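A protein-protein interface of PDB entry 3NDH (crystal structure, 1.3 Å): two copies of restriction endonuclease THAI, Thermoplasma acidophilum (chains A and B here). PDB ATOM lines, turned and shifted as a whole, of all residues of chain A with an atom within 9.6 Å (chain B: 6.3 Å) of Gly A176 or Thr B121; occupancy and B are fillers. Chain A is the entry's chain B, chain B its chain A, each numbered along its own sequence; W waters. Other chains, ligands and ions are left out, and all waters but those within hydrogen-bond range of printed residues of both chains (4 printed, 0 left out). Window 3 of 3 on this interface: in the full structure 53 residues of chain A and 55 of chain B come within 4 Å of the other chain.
Of the 10 printed residues of chain A, 5 touch a printed residue of chain B.
Printed residues of chain A that touch a printed residue of chain B: Val A118, Lys A174, Gln A175, Gly A176 and Thr A177.
Hydrophobic or aromatic side chains of chain A within 4 Å of the printed part of chain B: Val A118.
Of the 9 printed residues of chain B, 4 touch a printed residue of chain A.
Hydrophobic or aromatic side chains of chain B within 4 Å of the printed part of chain A: Val B118.
Along chain B the printed residues that touch a printed residue of chain A span positions 118 to 122.
Among the printed residues, 9 pairs touch across the chains.
The side-chain carboxylate (OD1) of Asp B119 lies within hydrogen-bond range of the backbone NH (N) of Gly A176 (2.9 Å).
OD1 of Asp B119 sits close to O of Thr A177 (3.3 Å).
Water W3 bridges the side-chain carboxylate of Asp B119 and the backbone carbonyl oxygen of Lys A174.
Water W4 lies within hydrogen-bond range of OD1 of Asn A178, N of Val B118, N of Asp B119 and O of Pro A179.
Water W1 lies within hydrogen-bond range of OD1 of Asp B119, OG1 of Thr B121 and N of Gly A176.
Water W2 bridges the backbone NH of Val B118 (3.2 Å) and the backbone carbonyl oxygen of Pro A179 (3.5 Å).
Val B118 touches its own counterpart, Val A118.
Positions printed for both chains: 118 and 120.
Of the printed residues of chain B, Val A118 touches Val B118 and Asp B119.
Leu A172 touches none of the printed residues of chain B.
Printed residues of chain B within 4 Å of Lys A174: Asp B119 (3.9999 Å).
Of chain B, only Asp B119 (2.9 Å), Thr B121 (3.96 Å) and Lys B122 (3.8 Å) come within 4 Å of Gly A176.
Of the printed residues of chain B, Thr A177 touches Asp B119 and Lys B122.
Printed residues of chain A within 4 Å of Val B118: Val A118.
Of the printed residues of chain A, Asp B119 touches Val A118 (3.7 Å), Lys A174 (3.9999 Å), Gln A175 (3.4 Å), Gly A176 (2.9 Å) and Thr A177 (2.9 Å).
Ala B120 touches none of the printed residues of chain A.
Thr B121 touches one residue of chain A.
Of chain A, only Gly A176 and Thr A177 come within 4 Å of Lys B122.
No residue of chain A comes within 4 Å of Ala B123.
The nearest printed residue of chain B that does not touch Gly A176 is Ala B120 (6.1 Å).
The nearest residue of chain A that does not touch Thr B121 is Gln A175 (5.3 Å).
The nearest printed residue of chain B that does not touch Lys A174 is Lys B122 (7.0 Å).
OD2 of Asp B119 is in hydrogen-bond range of N of Lys B122 (2.9 Å).
OD2 of Asp B119 lies within hydrogen-bond range of N of Thr B121 (3.2 Å).
O of Lys A174 is in hydrogen-bond range of OG1 of Thr A177, 2.7 Å away.
Val A118 touches Val B118 (CB to CB, 3.9 Å).
Val A118 touches Asp B119.
Lys A174 touches Asp B119.
Gln A175 touches Asp B119 (CA to OD1, 3.4 Å).
CB of Thr B121 touches CA of Gly A176 (3.96 Å).
O of Gly A176 touches CD of Lys B122, 3.8 Å away.
Lys B122 touches Thr A177 (CG to O, 3.6 Å).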
ATOM      1  N   VAL A 118      -5.476 -11.188  -6.062  1.00  0.00           N
ATOM      2  CA  VAL A 118      -5.903 -11.910  -7.255  1.00  0.00           C
ATOM      3  C   VAL A 118      -7.059 -12.867  -6.962  1.00  0.00           C
ATOM      4  O   VAL A 118      -7.892 -13.120  -7.841  1.00  0.00           O
ATOM      5  CB  VAL A 118      -4.712 -12.646  -7.872  1.00  0.00           C
ATOM      6  CG1 VAL A 118      -5.138 -13.538  -9.019  1.00  0.00           C
ATOM      7  CG2 VAL A 118      -3.678 -11.638  -8.328  1.00  0.00           C
ATOM      8  N   ALA A 120     -10.364 -14.559  -6.571  1.00  0.00           N
ATOM      9  CA  ALA A 120     -11.576 -14.087  -7.246  1.00  0.00           C
ATOM     10  C   ALA A 120     -12.601 -13.530  -6.279  1.00  0.00           C
ATOM     11  O   ALA A 120     -13.156 -12.462  -6.521  1.00  0.00           O
ATOM     12  CB  ALA A 120     -12.211 -15.192  -8.082  1.00  0.00           C
ATOM     13  N   LEU A 172     -11.524  -5.977 -12.270  1.00  0.00           N
ATOM     14  CA  LEU A 172     -11.176  -7.228 -11.598  1.00  0.00           C
ATOM     15  C   LEU A 172     -10.081  -7.997 -12.335  1.00  0.00           C
ATOM     16  O   LEU A 172      -9.941  -7.870 -13.562  1.00  0.00           O
ATOM     17  CB  LEU A 172     -12.408  -8.126 -11.441  1.00  0.00           C
ATOM     18  CG  LEU A 172     -13.556  -7.621 -10.570  1.00  0.00           C
ATOM     19  CD1 LEU A 172     -14.824  -8.473 -10.775  1.00  0.00           C
ATOM     20  CD2 LEU A 172     -13.136  -7.605  -9.117  1.00  0.00           C
ATOM     21  N   PRO A 173      -9.287  -8.786 -11.592  1.00  0.00           N
ATOM     22  CA  PRO A 173      -8.298  -9.627 -12.254  1.00  0.00           C
ATOM     23  C   PRO A 173      -8.997 -10.602 -13.191  1.00  0.00           C
ATOM     24  O   PRO A 173     -10.086 -11.092 -12.880  1.00  0.00           O
ATOM     25  CB  PRO A 173      -7.599 -10.354 -11.093  1.00  0.00           C
ATOM     26  CG  PRO A 173      -8.502 -10.211  -9.941  1.00  0.00           C
ATOM     27  CD  PRO A 173      -9.277  -8.964 -10.132  1.00  0.00           C
ATOM     28  N   LYS A 174      -8.411 -10.831 -14.361  1.00  0.00           N
ATOM     29  CA  LYS A 174      -9.043 -11.669 -15.371  1.00  0.00           C
ATOM     30  C   LYS A 174      -8.772 -13.135 -15.056  1.00  0.00           C
ATOM     31  O   LYS A 174      -7.616 -13.574 -15.008  1.00  0.00           O
ATOM     32  CB  LYS A 174      -8.540 -11.304 -16.772  1.00  0.00           C
ATOM     33  CG  LYS A 174      -9.126 -12.151 -17.884  1.00  0.00           C
ATOM     34  CD  LYS A 174      -9.085 -11.422 -19.223  1.00  0.00           C
ATOM     35  CE  LYS A 174      -9.348 -12.367 -20.383  1.00  0.00           C
ATOM     36  NZ  LYS A 174      -9.137 -11.714 -21.704  1.00  0.00           N
ATOM     37  N   GLN A 175      -9.842 -13.885 -14.820  1.00  0.00           N
ATOM     38  CA  GLN A 175      -9.723 -15.298 -14.482  1.00  0.00           C
ATOM     39  C   GLN A 175      -9.155 -16.080 -15.665  1.00  0.00           C
ATOM     40  O   GLN A 175      -9.434 -15.776 -16.832  1.00  0.00           O
ATOM     41  CB  GLN A 175     -11.063 -15.860 -13.989  1.00  0.00           C
ATOM     42  CG  GLN A 175     -11.443 -15.273 -12.621  1.00  0.00           C
ATOM     43  CD  GLN A 175     -12.792 -15.728 -12.111  1.00  0.00           C
ATOM     44  OE1 GLN A 175     -13.041 -16.923 -11.944  1.00  0.00           O
ATOM     45  NE2 GLN A 175     -13.662 -14.771 -11.831  1.00  0.00           N
ATOM     46  N   GLY A 176      -8.325 -17.063 -15.350  1.00  0.00           N
ATOM     47  CA  GLY A 176      -7.622 -17.854 -16.356  1.00  0.00           C
ATOM     48  C   GLY A 176      -6.338 -17.226 -16.878  1.00  0.00           C
ATOM     49  O   GLY A 176      -5.696 -17.791 -17.763  1.00  0.00           O
ATOM     50  N   THR A 177      -5.981 -16.048 -16.360  1.00  0.00           N
ATOM     51  CA  THR A 177      -4.698 -15.430 -16.639  1.00  0.00           C
ATOM     52  C   THR A 177      -3.960 -15.390 -15.316  1.00  0.00           C
ATOM     53  O   THR A 177      -4.526 -15.745 -14.282  1.00  0.00           O
ATOM     54  CB  THR A 177      -4.825 -14.007 -17.224  1.00  0.00           C
ATOM     55  OG1 THR A 177      -5.245 -13.087 -16.210  1.00  0.00           O
ATOM     56  CG2 THR A 177      -5.815 -13.986 -18.428  1.00  0.00           C
ATOM     57  N   ASN A 178      -2.708 -14.956 -15.364  1.00  0.00           N
ATOM     58  CA  ASN A 178      -1.868 -14.835 -14.175  1.00  0.00           C
ATOM     59  C   ASN A 178      -1.543 -13.367 -13.901  1.00  0.00           C
ATOM     60  O   ASN A 178      -0.467 -12.905 -14.272  1.00  0.00           O
ATOM     61  CB  ASN A 178      -0.597 -15.670 -14.379  1.00  0.00           C
ATOM     62  CG  ASN A 178       0.363 -15.597 -13.194  1.00  0.00           C
ATOM     63  OD1 ASN A 178       0.000 -15.162 -12.094  1.00  0.00           O
ATOM     64  ND2 ASN A 178       1.603 -16.012 -13.435  1.00  0.00           N
ATOM     65  N   PRO A 179      -2.492 -12.607 -13.314  1.00  0.00           N
ATOM     66  CA  PRO A 179      -2.283 -11.199 -13.060  1.00  0.00           C
ATOM     67  C   PRO A 179      -1.739 -10.952 -11.647  1.00  0.00           C
ATOM     68  O   PRO A 179      -1.386 -11.912 -10.931  1.00  0.00           O
ATOM     69  CB  PRO A 179      -3.692 -10.645 -13.215  1.00  0.00           C
ATOM     70  CG  PRO A 179      -4.555 -11.709 -12.595  1.00  0.00           C
ATOM     71  CD  PRO A 179      -3.853 -13.011 -12.898  1.00  0.00           C
ATOM     72  N   VAL B 118      -1.668 -16.980  -8.140  1.00  0.00           N
ATOM     73  CA  VAL B 118      -2.859 -17.158  -7.312  1.00  0.00           C
ATOM     74  C   VAL B 118      -4.105 -17.519  -8.137  1.00  0.00           C
ATOM     75  O   VAL B 118      -4.986 -18.221  -7.640  1.00  0.00           O
ATOM     76  CB  VAL B 118      -3.121 -15.899  -6.456  1.00  0.00           C
ATOM     77  CG1 VAL B 118      -4.448 -16.010  -5.740  1.00  0.00           C
ATOM     78  CG2 VAL B 118      -2.000 -15.730  -5.453  1.00  0.00           C
ATOM     79  N   ASP B 119      -4.161 -17.087  -9.397  1.00  0.00           N
ATOM     80  CA  ASP B 119      -5.285 -17.444 -10.258  1.00  0.00           C
ATOM     81  C   ASP B 119      -5.559 -18.940 -10.166  1.00  0.00           C
ATOM     82  O   ASP B 119      -4.656 -19.770 -10.341  1.00  0.00           O
ATOM     83  CB  ASP B 119      -5.033 -17.066 -11.714  1.00  0.00           C
ATOM     84  CG  ASP B 119      -6.174 -17.495 -12.619  1.00  0.00           C
ATOM     85  OD1 ASP B 119      -7.214 -16.793 -12.668  1.00  0.00           O
ATOM     86  OD2 ASP B 119      -6.039 -18.525 -13.284  1.00  0.00           O
ATOM     87  N   ALA B 120      -6.819 -19.297  -9.920  1.00  0.00           N
ATOM     88  CA  ALA B 120      -7.161 -20.690  -9.621  1.00  0.00           C
ATOM     89  C   ALA B 120      -6.860 -21.612 -10.801  1.00  0.00           C
ATOM     90  O   ALA B 120      -6.322 -22.700 -10.631  1.00  0.00           O
ATOM     91  CB  ALA B 120      -8.631 -20.821  -9.197  1.00  0.00           C
ATOM     92  N   THR B 121      -7.236 -21.178 -12.001  1.00  0.00           N
ATOM     93  CA  THR B 121      -7.038 -21.978 -13.205  1.00  0.00           C
ATOM     94  C   THR B 121      -5.553 -22.190 -13.479  1.00  0.00           C
ATOM     95  O   THR B 121      -5.105 -23.313 -13.697  1.00  0.00           O
ATOM     96  CB  THR B 121      -7.722 -21.304 -14.422  1.00  0.00           C
ATOM     97  OG1 THR B 121      -9.116 -21.133 -14.150  1.00  0.00           O
ATOM     98  CG2 THR B 121      -7.565 -22.132 -15.685  1.00  0.00           C
ATOM     99  N   LYS B 122      -4.784 -21.107 -13.464  1.00  0.00           N
ATOM    100  CA  LYS B 122      -3.336 -21.207 -13.695  1.00  0.00           C
ATOM    101  C   LYS B 122      -2.621 -22.020 -12.595  1.00  0.00           C
ATOM    102  O   LYS B 122      -1.698 -22.780 -12.885  1.00  0.00           O
ATOM    103  CB  LYS B 122      -2.718 -19.819 -13.816  1.00  0.00           C
ATOM    104  CG  LYS B 122      -3.152 -18.996 -15.034  1.00  0.00           C
ATOM    105  CD  LYS B 122      -2.636 -19.540 -16.346  1.00  0.00           C
ATOM    106  CE  LYS B 122      -1.142 -19.388 -16.504  1.00  0.00           C
ATOM    107  NZ  LYS B 122      -0.734 -19.671 -17.917  1.00  0.00           N
ATOM    108  N   ALA B 123      -3.056 -21.874 -11.344  1.00  0.00           N
ATOM    109  CA  ALA B 123      -2.503 -22.677 -10.245  1.00  0.00           C
ATOM    110  C   ALA B 123      -2.727 -24.176 -10.448  1.00  0.00           C
ATOM    111  O   ALA B 123      -1.827 -24.973 -10.216  1.00  0.00           O
ATOM    112  CB  ALA B 123      -3.075 -22.226  -8.913  1.00  0.00           C
ATOM    113  N   ARG B 124      -3.920 -24.557 -10.879  1.00  0.00           N
ATOM    114  CA  ARG B 124      -4.209 -25.967 -11.134  1.00  0.00           C
ATOM    115  C   ARG B 124      -3.417 -26.482 -12.337  1.00  0.00           C
ATOM    116  O   ARG B 124      -2.974 -27.624 -12.351  1.00  0.00           O
ATOM    117  CB  ARG B 124      -5.711 -26.188 -11.310  1.00  0.00           C
ATOM    118  CG  ARG B 124      -6.103 -27.645 -11.483  1.00  0.00           C
ATOM    119  CD  ARG B 124      -7.424 -27.956 -10.792  1.00  0.00           C
ATOM    120  NE  ARG B 124      -7.250 -28.173  -9.349  1.00  0.00           N
ATOM    121  CZ  ARG B 124      -7.322 -29.354  -8.729  1.00  0.00           C
ATOM    122  NH1 ARG B 124      -7.155 -29.416  -7.413  1.00  0.00           N
ATOM    123  NH2 ARG B 124      -7.565 -30.478  -9.399  1.00  0.00           N
ATOM    124  N   GLN B 125      -3.206 -25.627 -13.329  1.00  0.00           N
ATOM    125  CA  GLN B 125      -2.344 -25.967 -14.464  1.00  0.00           C
ATOM    126  C   GLN B 125      -0.920 -26.268 -14.006  1.00  0.00           C
ATOM    127  O   GLN B 125      -0.291 -27.210 -14.483  1.00  0.00           O
ATOM    128  CB  GLN B 125      -2.328 -24.821 -15.475  1.00  0.00           C
ATOM    129  CG  GLN B 125      -1.595 -25.124 -16.767  1.00  0.00           C
ATOM    130  CD  GLN B 125      -1.683 -23.987 -17.760  1.00  0.00           C
ATOM    131  OE1 GLN B 125      -2.677 -23.260 -17.806  1.00  0.00           O
ATOM    132  NE2 GLN B 125      -0.646 -23.835 -18.575  1.00  0.00           N
ATOM    133  N   PHE B 126      -0.406 -25.453 -13.092  1.00  0.00           N
ATOM    134  CA  PHE B 126       0.905 -25.698 -12.495  1.00  0.00           C
ATOM    135  C   PHE B 126       0.949 -27.046 -11.773  1.00  0.00           C
ATOM    136  O   PHE B 126       1.861 -27.847 -12.001  1.00  0.00           O
ATOM    137  CB  PHE B 126       1.260 -24.560 -11.533  1.00  0.00           C
ATOM    138  CG  PHE B 126       2.611 -24.696 -10.889  1.00  0.00           C
ATOM    139  CD1 PHE B 126       3.747 -24.148 -11.489  1.00  0.00           C
ATOM    140  CD2 PHE B 126       2.751 -25.325  -9.664  1.00  0.00           C
ATOM    141  CE1 PHE B 126       4.983 -24.272 -10.894  1.00  0.00           C
ATOM    142  CE2 PHE B 126       3.998 -25.455  -9.081  1.00  0.00           C
ATOM    143  CZ  PHE B 126       5.097 -24.911  -9.691  1.00  0.00           C
HETATM  144  O   HOH W   1      -9.182 -18.780 -12.593  1.00  0.00           O
HETATM  145  O   HOH W   2      -0.567 -14.003  -8.272  1.00  0.00           O
HETATM  146  O   HOH W   3      -7.049 -14.165 -12.114  1.00  0.00           O
HETATM  147  O   HOH W   4      -2.091 -15.081 -10.395  1.00  0.00           O
